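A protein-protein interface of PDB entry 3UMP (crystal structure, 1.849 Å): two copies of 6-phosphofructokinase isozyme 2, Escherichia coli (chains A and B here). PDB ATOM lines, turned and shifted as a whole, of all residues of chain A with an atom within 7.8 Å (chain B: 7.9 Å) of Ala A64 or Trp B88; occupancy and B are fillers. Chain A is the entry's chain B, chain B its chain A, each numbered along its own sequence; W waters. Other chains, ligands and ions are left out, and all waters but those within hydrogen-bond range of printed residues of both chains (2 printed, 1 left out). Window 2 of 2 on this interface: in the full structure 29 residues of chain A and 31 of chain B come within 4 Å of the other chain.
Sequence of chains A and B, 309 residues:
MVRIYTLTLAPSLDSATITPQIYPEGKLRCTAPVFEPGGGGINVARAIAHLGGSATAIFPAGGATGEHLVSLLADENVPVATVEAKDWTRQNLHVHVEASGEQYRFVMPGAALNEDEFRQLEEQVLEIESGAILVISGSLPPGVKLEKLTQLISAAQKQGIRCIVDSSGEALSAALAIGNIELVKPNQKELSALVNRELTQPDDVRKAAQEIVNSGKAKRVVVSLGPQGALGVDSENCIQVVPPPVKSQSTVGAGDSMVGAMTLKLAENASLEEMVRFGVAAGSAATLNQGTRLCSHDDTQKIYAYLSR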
ATOM      1  N   LEU A  13      29.834 -21.398   0.644  1.00  0.00           N
ATOM      2  CA  LEU A  13      30.198 -21.410  -0.757  1.00  0.00           C
ATOM      3  C   LEU A  13      30.175 -19.955  -1.164  1.00  0.00           C
ATOM      4  O   LEU A  13      29.108 -19.374  -1.338  1.00  0.00           O
ATOM      5  CB  LEU A  13      29.192 -22.204  -1.593  1.00  0.00           C
ATOM      6  CG  LEU A  13      29.623 -22.301  -3.056  1.00  0.00           C
ATOM      7  CD1 LEU A  13      30.897 -23.146  -3.143  1.00  0.00           C
ATOM      8  CD2 LEU A  13      28.509 -22.875  -3.922  1.00  0.00           C
ATOM      9  N   SER A  15      30.679 -16.525  -3.392  1.00  0.00           N
ATOM     10  CA  SER A  15      30.618 -16.040  -4.766  1.00  0.00           C
ATOM     11  C   SER A  15      31.539 -14.838  -4.956  1.00  0.00           C
ATOM     12  O   SER A  15      31.507 -13.888  -4.173  1.00  0.00           O
ATOM     13  CB  SER A  15      29.196 -15.626  -5.123  1.00  0.00           C
ATOM     14  OG  SER A  15      28.397 -16.754  -5.396  1.00  0.00           O
ATOM     15  N   PRO A  33      29.204 -15.427 -11.165  1.00  0.00           N
ATOM     16  CA  PRO A  33      30.193 -15.562 -10.088  1.00  0.00           C
ATOM     17  C   PRO A  33      31.112 -16.771 -10.236  1.00  0.00           C
ATOM     18  O   PRO A  33      30.740 -17.795 -10.835  1.00  0.00           O
ATOM     19  CB  PRO A  33      29.329 -15.717  -8.832  1.00  0.00           C
ATOM     20  CG  PRO A  33      28.034 -16.278  -9.337  1.00  0.00           C
ATOM     21  CD  PRO A  33      27.826 -15.637 -10.689  1.00  0.00           C
ATOM     22  N   PHE A  35      32.819 -19.504  -7.909  1.00  0.00           N
ATOM     23  CA  PHE A  35      32.575 -20.040  -6.573  1.00  0.00           C
ATOM     24  C   PHE A  35      33.886 -20.488  -5.920  1.00  0.00           C
ATOM     25  O   PHE A  35      34.742 -21.054  -6.589  1.00  0.00           O
ATOM     26  CB  PHE A  35      31.564 -21.190  -6.649  1.00  0.00           C
ATOM     27  CG  PHE A  35      30.213 -20.768  -7.157  1.00  0.00           C
ATOM     28  CD1 PHE A  35      29.431 -19.883  -6.424  1.00  0.00           C
ATOM     29  CD2 PHE A  35      29.725 -21.254  -8.361  1.00  0.00           C
ATOM     30  CE1 PHE A  35      28.192 -19.483  -6.883  1.00  0.00           C
ATOM     31  CE2 PHE A  35      28.483 -20.859  -8.835  1.00  0.00           C
ATOM     32  CZ  PHE A  35      27.714 -19.975  -8.099  1.00  0.00           C
ATOM     33  N   ALA A  61      27.955 -30.023   5.337  1.00  0.00           N
ATOM     34  CA  ALA A  61      27.631 -29.593   3.976  1.00  0.00           C
ATOM     35  C   ALA A  61      26.172 -29.884   3.664  1.00  0.00           C
ATOM     36  O   ALA A  61      25.679 -30.973   3.955  1.00  0.00           O
ATOM     37  CB  ALA A  61      28.540 -30.301   2.950  1.00  0.00           C
ATOM     38  N   GLY A  62      25.481 -28.922   3.058  1.00  0.00           N
ATOM     39  CA  GLY A  62      24.068 -29.095   2.765  1.00  0.00           C
ATOM     40  C   GLY A  62      23.656 -28.624   1.383  1.00  0.00           C
ATOM     41  O   GLY A  62      24.074 -27.561   0.925  1.00  0.00           O
ATOM     42  N   GLY A  63      22.833 -29.426   0.713  1.00  0.00           N
ATOM     43  CA  GLY A  63      22.273 -29.040  -0.573  1.00  0.00           C
ATOM     44  C   GLY A  63      23.283 -28.956  -1.704  1.00  0.00           C
ATOM     45  O   GLY A  63      24.447 -29.351  -1.558  1.00  0.00           O
ATOM     46  N   ALA A  64      22.830 -28.439  -2.843  1.00  0.00           N
ATOM     47  CA  ALA A  64      23.675 -28.321  -4.033  1.00  0.00           C
ATOM     48  C   ALA A  64      24.887 -27.426  -3.785  1.00  0.00           C
ATOM     49  O   ALA A  64      25.957 -27.641  -4.357  1.00  0.00           O
ATOM     50  CB  ALA A  64      22.859 -27.811  -5.224  1.00  0.00           C
ATOM     51  N   THR A  65      24.719 -26.413  -2.945  1.00  0.00           N
ATOM     52  CA  THR A  65      25.832 -25.522  -2.648  1.00  0.00           C
ATOM     53  C   THR A  65      26.892 -26.279  -1.847  1.00  0.00           C
ATOM     54  O   THR A  65      28.099 -26.102  -2.059  1.00  0.00           O
ATOM     55  CB  THR A  65      25.365 -24.260  -1.899  1.00  0.00           C
ATOM     56  OG1 THR A  65      24.509 -24.639  -0.812  1.00  0.00           O
ATOM     57  CG2 THR A  65      24.602 -23.342  -2.836  1.00  0.00           C
ATOM     58  N   GLY A  66      26.436 -27.140  -0.940  1.00  0.00           N
ATOM     59  CA  GLY A  66      27.346 -27.961  -0.160  1.00  0.00           C
ATOM     60  C   GLY A  66      28.113 -28.952  -1.019  1.00  0.00           C
ATOM     61  O   GLY A  66      29.297 -29.200  -0.791  1.00  0.00           O
ATOM     62  N   GLU A  67      27.431 -29.527  -2.006  1.00  0.00           N
ATOM     63  CA  GLU A  67      28.059 -30.480  -2.910  1.00  0.00           C
ATOM     64  C   GLU A  67      29.131 -29.774  -3.729  1.00  0.00           C
ATOM     65  O   GLU A  67      30.192 -30.339  -3.991  1.00  0.00           O
ATOM     66  CB  GLU A  67      27.028 -31.103  -3.861  1.00  0.00           C
ATOM     67  CG  GLU A  67      25.936 -31.930  -3.187  1.00  0.00           C
ATOM     68  CD  GLU A  67      24.818 -32.314  -4.153  1.00  0.00           C
ATOM     69  OE1 GLU A  67      23.649 -32.401  -3.709  1.00  0.00           O
ATOM     70  OE2 GLU A  67      25.109 -32.524  -5.354  1.00  0.00           O
ATOM     71  N   HIS A  68      28.851 -28.540  -4.141  1.00  0.00           N
ATOM     72  CA  HIS A  68      29.816 -27.799  -4.953  1.00  0.00           C
ATOM     73  C   HIS A  68      31.029 -27.390  -4.122  1.00  0.00           C
ATOM     74  O   HIS A  68      32.155 -27.380  -4.618  1.00  0.00           O
ATOM     75  CB  HIS A  68      29.178 -26.576  -5.615  1.00  0.00           C
ATOM     76  CG  HIS A  68      29.986 -26.023  -6.748  1.00  0.00           C
ATOM     77  ND1 HIS A  68      30.368 -26.790  -7.831  1.00  0.00           N
ATOM     78  CD2 HIS A  68      30.493 -24.788  -6.964  1.00  0.00           C
ATOM     79  CE1 HIS A  68      31.073 -26.046  -8.665  1.00  0.00           C
ATOM     80  NE2 HIS A  68      31.160 -24.824  -8.164  1.00  0.00           N
ATOM     81  N   LEU A  69      30.799 -27.061  -2.856  1.00  0.00           N
ATOM     82  CA  LEU A  69      31.896 -26.777  -1.935  1.00  0.00           C
ATOM     83  C   LEU A  69      32.832 -27.975  -1.806  1.00  0.00           C
ATOM     84  O   LEU A  69      34.056 -27.831  -1.859  1.00  0.00           O
ATOM     85  CB  LEU A  69      31.348 -26.367  -0.559  1.00  0.00           C
ATOM     86  CG  LEU A  69      32.295 -26.217   0.642  1.00  0.00           C
ATOM     87  CD1 LEU A  69      33.407 -25.232   0.387  1.00  0.00           C
ATOM     88  CD2 LEU A  69      31.522 -25.789   1.878  1.00  0.00           C
ATOM     89  N   VAL A  70      32.255 -29.160  -1.635  1.00  0.00           N
ATOM     90  CA  VAL A  70      33.050 -30.370  -1.510  1.00  0.00           C
ATOM     91  C   VAL A  70      33.791 -30.629  -2.822  1.00  0.00           C
ATOM     92  O   VAL A  70      34.960 -31.037  -2.820  1.00  0.00           O
ATOM     93  CB  VAL A  70      32.169 -31.572  -1.109  1.00  0.00           C
ATOM     94  CG1 VAL A  70      32.904 -32.884  -1.323  1.00  0.00           C
ATOM     95  CG2 VAL A  70      31.712 -31.429   0.352  1.00  0.00           C
ATOM     96  N   SER A  71      33.108 -30.350  -3.932  1.00  0.00           N
ATOM     97  CA  SER A  71      33.661 -30.555  -5.271  1.00  0.00           C
ATOM     98  C   SER A  71      34.891 -29.685  -5.503  1.00  0.00           C
ATOM     99  O   SER A  71      35.895 -30.137  -6.060  1.00  0.00           O
ATOM    100  CB  SER A  71      32.607 -30.244  -6.338  1.00  0.00           C
ATOM    101  OG  SER A  71      32.781 -31.081  -7.459  1.00  0.00           O
ATOM    102  N   TRP A  88      20.848 -25.711   3.876  1.00  0.00           N
ATOM    103  CA  TRP A  88      21.798 -25.639   2.772  1.00  0.00           C
ATOM    104  C   TRP A  88      22.979 -24.717   3.075  1.00  0.00           C
ATOM    105  O   TRP A  88      22.826 -23.687   3.731  1.00  0.00           O
ATOM    106  CB  TRP A  88      21.108 -25.254   1.455  1.00  0.00           C
ATOM    107  CG  TRP A  88      20.824 -23.775   1.289  1.00  0.00           C
ATOM    108  CD1 TRP A  88      21.700 -22.802   0.877  1.00  0.00           C
ATOM    109  CD2 TRP A  88      19.577 -23.115   1.514  1.00  0.00           C
ATOM    110  NE1 TRP A  88      21.074 -21.580   0.845  1.00  0.00           N
ATOM    111  CE2 TRP A  88      19.770 -21.745   1.231  1.00  0.00           C
ATOM    112  CE3 TRP A  88      18.320 -23.547   1.940  1.00  0.00           C
ATOM    113  CZ2 TRP A  88      18.751 -20.808   1.358  1.00  0.00           C
ATOM    114  CZ3 TRP A  88      17.307 -22.617   2.065  1.00  0.00           C
ATOM    115  CH2 TRP A  88      17.527 -21.262   1.776  1.00  0.00           C
ATOM    116  N   THR A  89      24.156 -25.103   2.589  1.00  0.00           N
ATOM    117  CA  THR A  89      25.384 -24.327   2.765  1.00  0.00           C
ATOM    118  C   THR A  89      25.212 -22.890   2.239  1.00  0.00           C
ATOM    119  O   THR A  89      24.864 -22.683   1.071  1.00  0.00           O
ATOM    120  CB  THR A  89      26.565 -25.042   2.061  1.00  0.00           C
ATOM    121  OG1 THR A  89      26.800 -26.300   2.706  1.00  0.00           O
ATOM    122  CG2 THR A  89      27.843 -24.201   2.092  1.00  0.00           C
ATOM    123  N   GLN A  91      25.971 -18.707   1.394  1.00  0.00           N
ATOM    124  CA  GLN A  91      26.875 -18.037   0.467  1.00  0.00           C
ATOM    125  C   GLN A  91      27.199 -16.627   0.928  1.00  0.00           C
ATOM    126  O   GLN A  91      26.290 -15.850   1.231  1.00  0.00           O
ATOM    127  CB  GLN A  91      26.229 -17.938  -0.912  1.00  0.00           C
ATOM    128  CG  GLN A  91      25.840 -19.269  -1.521  1.00  0.00           C
ATOM    129  CD  GLN A  91      25.526 -19.149  -3.001  1.00  0.00           C
ATOM    130  OE1 GLN A  91      24.367 -19.024  -3.395  1.00  0.00           O
ATOM    131  NE2 GLN A  91      26.566 -19.181  -3.829  1.00  0.00           N
ATOM    132  N   PRO B  11      14.692 -17.010 -12.611  1.00  0.00           N
ATOM    133  CA  PRO B  11      14.266 -16.623 -11.260  1.00  0.00           C
ATOM    134  C   PRO B  11      15.425 -16.579 -10.263  1.00  0.00           C
ATOM    135  O   PRO B  11      16.538 -17.034 -10.543  1.00  0.00           O
ATOM    136  CB  PRO B  11      13.319 -17.750 -10.859  1.00  0.00           C
ATOM    137  CG  PRO B  11      13.814 -18.932 -11.601  1.00  0.00           C
ATOM    138  CD  PRO B  11      14.340 -18.410 -12.920  1.00  0.00           C
ATOM    139  N   PRO B  60      11.638 -22.255 -13.843  1.00  0.00           N
ATOM    140  CA  PRO B  60      12.468 -23.379 -13.399  1.00  0.00           C
ATOM    141  C   PRO B  60      12.931 -23.180 -11.954  1.00  0.00           C
ATOM    142  O   PRO B  60      13.302 -22.064 -11.565  1.00  0.00           O
ATOM    143  CB  PRO B  60      13.675 -23.288 -14.324  1.00  0.00           C
ATOM    144  CG  PRO B  60      13.818 -21.779 -14.574  1.00  0.00           C
ATOM    145  CD  PRO B  60      12.389 -21.309 -14.697  1.00  0.00           C
ATOM    146  N   ALA B  61      12.925 -24.257 -11.180  1.00  0.00           N
ATOM    147  CA  ALA B  61      13.428 -24.230  -9.810  1.00  0.00           C
ATOM    148  C   ALA B  61      14.386 -25.389  -9.595  1.00  0.00           C
ATOM    149  O   ALA B  61      14.114 -26.514 -10.020  1.00  0.00           O
ATOM    150  CB  ALA B  61      12.277 -24.324  -8.831  1.00  0.00           C
ATOM    151  N   GLY B  62      15.499 -25.124  -8.918  1.00  0.00           N
ATOM    152  CA  GLY B  62      16.484 -26.163  -8.670  1.00  0.00           C
ATOM    153  C   GLY B  62      17.044 -26.125  -7.262  1.00  0.00           C
ATOM    154  O   GLY B  62      17.261 -25.050  -6.702  1.00  0.00           O
ATOM    155  N   GLY B  63      17.272 -27.305  -6.692  1.00  0.00           N
ATOM    156  CA  GLY B  63      17.913 -27.430  -5.396  1.00  0.00           C
ATOM    157  C   GLY B  63      17.111 -26.867  -4.243  1.00  0.00           C
ATOM    158  O   GLY B  63      15.930 -26.538  -4.382  1.00  0.00           O
ATOM    159  N   ALA B  64      17.771 -26.744  -3.096  1.00  0.00           N
ATOM    160  CA  ALA B  64      17.122 -26.289  -1.872  1.00  0.00           C
ATOM    161  C   ALA B  64      16.675 -24.834  -1.967  1.00  0.00           C
ATOM    162  O   ALA B  64      15.656 -24.462  -1.397  1.00  0.00           O
ATOM    163  CB  ALA B  64      18.041 -26.498  -0.670  1.00  0.00           C
ATOM    164  N   THR B  65      17.435 -24.008  -2.682  1.00  0.00           N
ATOM    165  CA  THR B  65      17.039 -22.618  -2.879  1.00  0.00           C
ATOM    166  C   THR B  65      15.760 -22.528  -3.703  1.00  0.00           C
ATOM    167  O   THR B  65      14.879 -21.707  -3.421  1.00  0.00           O
ATOM    168  CB  THR B  65      18.151 -21.773  -3.556  1.00  0.00           C
ATOM    169  OG1 THR B  65      18.625 -22.438  -4.736  1.00  0.00           O
ATOM    170  CG2 THR B  65      19.316 -21.560  -2.612  1.00  0.00           C
ATOM    171  N   GLY B  66      15.658 -23.374  -4.724  1.00  0.00           N
ATOM    172  CA  GLY B  66      14.463 -23.424  -5.545  1.00  0.00           C
ATOM    173  C   GLY B  66      13.257 -23.877  -4.749  1.00  0.00           C
ATOM    174  O   GLY B  66      12.151 -23.358  -4.927  1.00  0.00           O
ATOM    175  N   ALA B  85      14.966 -27.995 -12.346  1.00  0.00           N
ATOM    176  CA  ALA B  85      16.187 -27.790 -13.132  1.00  0.00           C
ATOM    177  C   ALA B  85      17.397 -28.400 -12.424  1.00  0.00           C
ATOM    178  O   ALA B  85      17.425 -28.473 -11.192  1.00  0.00           O
ATOM    179  CB  ALA B  85      16.409 -26.300 -13.390  1.00  0.00           C
ATOM    180  N   LYS B  86      18.397 -28.829 -13.196  1.00  0.00           N
ATOM    181  CA  LYS B  86      19.621 -29.399 -12.621  1.00  0.00           C
ATOM    182  C   LYS B  86      20.443 -28.363 -11.858  1.00  0.00           C
ATOM    183  O   LYS B  86      20.999 -28.662 -10.798  1.00  0.00           O
ATOM    184  CB  LYS B  86      20.500 -30.033 -13.702  1.00  0.00           C
ATOM    185  CG  LYS B  86      19.792 -31.080 -14.543  1.00  0.00           C
ATOM    186  CD  LYS B  86      20.519 -32.416 -14.484  1.00  0.00           C
ATOM    187  CE  LYS B  86      19.681 -33.532 -15.100  1.00  0.00           C
ATOM    188  NZ  LYS B  86      18.412 -33.752 -14.343  1.00  0.00           N
ATOM    189  N   ASP B  87      20.541 -27.155 -12.404  1.00  0.00           N
ATOM    190  CA  ASP B  87      21.356 -26.119 -11.777  1.00  0.00           C
ATOM    191  C   ASP B  87      20.537 -25.420 -10.691  1.00  0.00           C
ATOM    192  O   ASP B  87      19.391 -25.039 -10.927  1.00  0.00           O
ATOM    193  CB  ASP B  87      21.845 -25.120 -12.830  1.00  0.00           C
ATOM    194  CG  ASP B  87      23.077 -24.335 -12.376  1.00  0.00           C
ATOM    195  OD1 ASP B  87      23.654 -24.669 -11.320  1.00  0.00           O
ATOM    196  OD2 ASP B  87      23.471 -23.387 -13.090  1.00  0.00           O
ATOM    197  N   TRP B  88      21.119 -25.263  -9.504  1.00  0.00           N
ATOM    198  CA  TRP B  88      20.381 -24.726  -8.355  1.00  0.00           C
ATOM    199  C   TRP B  88      19.981 -23.256  -8.532  1.00  0.00           C
ATOM    200  O   TRP B  88      20.737 -22.450  -9.085  1.00  0.00           O
ATOM    201  CB  TRP B  88      21.173 -24.924  -7.040  1.00  0.00           C
ATOM    202  CG  TRP B  88      22.287 -23.915  -6.798  1.00  0.00           C
ATOM    203  CD1 TRP B  88      22.161 -22.639  -6.292  1.00  0.00           C
ATOM    204  CD2 TRP B  88      23.688 -24.112  -7.025  1.00  0.00           C
ATOM    205  NE1 TRP B  88      23.395 -22.035  -6.216  1.00  0.00           N
ATOM    206  CE2 TRP B  88      24.346 -22.918  -6.657  1.00  0.00           C
ATOM    207  CE3 TRP B  88      24.446 -25.177  -7.519  1.00  0.00           C
ATOM    208  CZ2 TRP B  88      25.728 -22.764  -6.765  1.00  0.00           C
ATOM    209  CZ3 TRP B  88      25.820 -25.024  -7.624  1.00  0.00           C
ATOM    210  CH2 TRP B  88      26.445 -23.826  -7.249  1.00  0.00           C
ATOM    211  N   THR B  89      18.786 -22.912  -8.057  1.00  0.00           N
ATOM    212  CA  THR B  89      18.290 -21.539  -8.153  1.00  0.00           C
ATOM    213  C   THR B  89      19.262 -20.548  -7.517  1.00  0.00           C
ATOM    214  O   THR B  89      19.676 -20.728  -6.360  1.00  0.00           O
ATOM    215  CB  THR B  89      16.881 -21.405  -7.536  1.00  0.00           C
ATOM    216  OG1 THR B  89      15.966 -22.200  -8.305  1.00  0.00           O
ATOM    217  CG2 THR B  89      16.408 -19.929  -7.554  1.00  0.00           C
ATOM    218  N   ARG B  90      19.633 -19.520  -8.287  1.00  0.00           N
ATOM    219  CA  ARG B  90      20.660 -18.555  -7.878  1.00  0.00           C
ATOM    220  C   ARG B  90      20.100 -17.464  -6.970  1.00  0.00           C
ATOM    221  O   ARG B  90      18.880 -17.323  -6.834  1.00  0.00           O
ATOM    222  CB  ARG B  90      21.331 -17.930  -9.103  1.00  0.00           C
ATOM    223  CG  ARG B  90      22.129 -18.915  -9.954  1.00  0.00           C
ATOM    224  CD  ARG B  90      23.299 -19.488  -9.151  1.00  0.00           C
ATOM    225  NE  ARG B  90      24.315 -20.120  -9.992  1.00  0.00           N
ATOM    226  CZ  ARG B  90      24.372 -21.423 -10.260  1.00  0.00           C
ATOM    227  NH1 ARG B  90      25.345 -21.900 -11.026  1.00  0.00           N
ATOM    228  NH2 ARG B  90      23.461 -22.256  -9.764  1.00  0.00           N
ATOM    229  N   GLN B  91      21.002 -16.698  -6.348  1.00  0.00           N
ATOM    230  CA  GLN B  91      20.622 -15.709  -5.338  1.00  0.00           C
ATOM    231  C   GLN B  91      21.213 -14.344  -5.636  1.00  0.00           C
ATOM    232  O   GLN B  91      22.421 -14.224  -5.855  1.00  0.00           O
ATOM    233  CB  GLN B  91      21.123 -16.130  -3.959  1.00  0.00           C
ATOM    234  CG  GLN B  91      20.723 -17.536  -3.523  1.00  0.00           C
ATOM    235  CD  GLN B  91      20.948 -17.745  -2.038  1.00  0.00           C
ATOM    236  OE1 GLN B  91      20.224 -17.192  -1.208  1.00  0.00           O
ATOM    237  NE2 GLN B  91      21.968 -18.527  -1.695  1.00  0.00           N
ATOM    238  N   PRO B 109      23.518 -13.382 -12.709  1.00  0.00           N
ATOM    239  CA  PRO B 109      22.678 -14.131 -13.654  1.00  0.00           C
ATOM    240  C   PRO B 109      21.886 -15.246 -12.988  1.00  0.00           C
ATOM    241  O   PRO B 109      22.258 -15.738 -11.915  1.00  0.00           O
ATOM    242  CB  PRO B 109      23.693 -14.749 -14.622  1.00  0.00           C
ATOM    243  CG  PRO B 109      24.944 -13.913 -14.482  1.00  0.00           C
ATOM    244  CD  PRO B 109      24.955 -13.493 -13.037  1.00  0.00           C
ATOM    245  N   GLY B 110      20.796 -15.645 -13.634  1.00  0.00           N
ATOM    246  CA  GLY B 110      20.026 -16.778 -13.155  1.00  0.00           C
ATOM    247  C   GLY B 110      20.772 -18.080 -13.390  1.00  0.00           C
ATOM    248  O   GLY B 110      21.794 -18.119 -14.086  1.00  0.00           O
ATOM    249  N   ALA B 111      20.257 -19.159 -12.814  1.00  0.00           N
ATOM    250  CA  ALA B 111      20.855 -20.474 -13.007  1.00  0.00           C
ATOM    251  C   ALA B 111      20.797 -20.868 -14.473  1.00  0.00           C
ATOM    252  O   ALA B 111      19.971 -20.359 -15.242  1.00  0.00           O
ATOM    253  CB  ALA B 111      20.143 -21.506 -12.168  1.00  0.00           C
ATOM    254  N   ALA B 112      21.674 -21.789 -14.854  1.00  0.00           N
ATOM    255  CA  ALA B 112      21.703 -22.287 -16.222  1.00  0.00           C
ATOM    256  C   ALA B 112      20.463 -23.129 -16.519  1.00  0.00           C
ATOM    257  O   ALA B 112      19.884 -23.752 -15.619  1.00  0.00           O
ATOM    258  CB  ALA B 112      22.979 -23.090 -16.486  1.00  0.00           C
HETATM  259  O   HOH W   1      19.937 -28.518  -2.903  1.00  0.00           O
HETATM  260  O   HOH W   2      23.012 -17.989   1.016  1.00  0.00           O
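The side-chain amide nitrogen (NE2) of Gln B91 is in hydrogen-bond range of the side-chain amide oxygen (OE1) of Gln A91 (3.0 Å).
OG1 of Thr B65 is in hydrogen-bond range of O of Thr B89, at 2.6 Å.
NH2 of Arg B90 lies within salt-bridge range of OD1 of Asp B87.
NH2 of Arg B90 sits at hydrogen-bond distance from O of Trp B88 (2.8 Å).
The side-chain hydroxyl of Ser A15 sits at hydrogen-bond distance from the side-chain amide nitrogen of Gln A91.
O of Gly A62 sits at hydrogen-bond distance from OG1 of Thr A65 (3.4 Å).
The side-chain hydroxyl of Thr A65 sits at hydrogen-bond distance from the backbone carbonyl oxygen of Thr A89.
Leu A13 touches Trp B88.
Trp B88 touches Phe A35 (CZ2 to CZ, 3.7 Å).
Phe A35 touches Arg B90 (CZ to NE, 3.9 Å).
CB of Ala A64 touches CB of Trp B88 (3.8 Å).
CG2 of Thr A65 touches NE1 of Trp B88, 3.8 Å away.
Ala B64 touches Trp A88.
Thr B65 touches Trp A88 (CG2 to CE2, 3.9 Å).
Of the printed residues of chain B, Thr A65 touches Trp B88.
Ala B61 touches none of the printed residues of chain A.
Printed residues of chain A within 4 Å of Ala B64: Trp A88 (3.9 Å).
Lys B86 touches none of the printed residues of chain A.
Trp B88 touches just these residues of chain A: Leu A13, Phe A35, Ala A64 and Thr A65.
The nearest residue of chain A that does not touch Trp B88 is His A68 (4.2 Å).
Along chain A the printed residues that touch a printed residue of chain B span positions 13 to 91.
Of the 19 printed residues of chain B, 5 touch a printed residue of chain A.
Among the printed residues, 8 pairs touch across the chains.
Among the printed residues, no Asp or Glu carboxylate lies within 4 Å of a Lys or Arg side-chain nitrogen of the other chain.
Ala A64 touches Trp B88, and with the chains exchanged Trp A88 touches Ala B64.
Thr A65 touches Trp B88, and with the chains exchanged Trp A88 touches Thr B65.
Gln B91 touches its own counterpart, Gln A91.
Positions printed for both chains: 61, 62, 63, 64, 65, 66, 88, 89 and 91.
Of the 8 pairs that touch across the chains among the printed residues, 5 have their exchanged pair printed and touching as well.
Water W1 lies within hydrogen-bond range of N of Ala B64 (2.8 Å) and N of Ala A64 (2.9 Å).
Water W2 bridges NE2 of Gln B91 (3.0 Å) and N of Gln A91 (3.1 Å).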
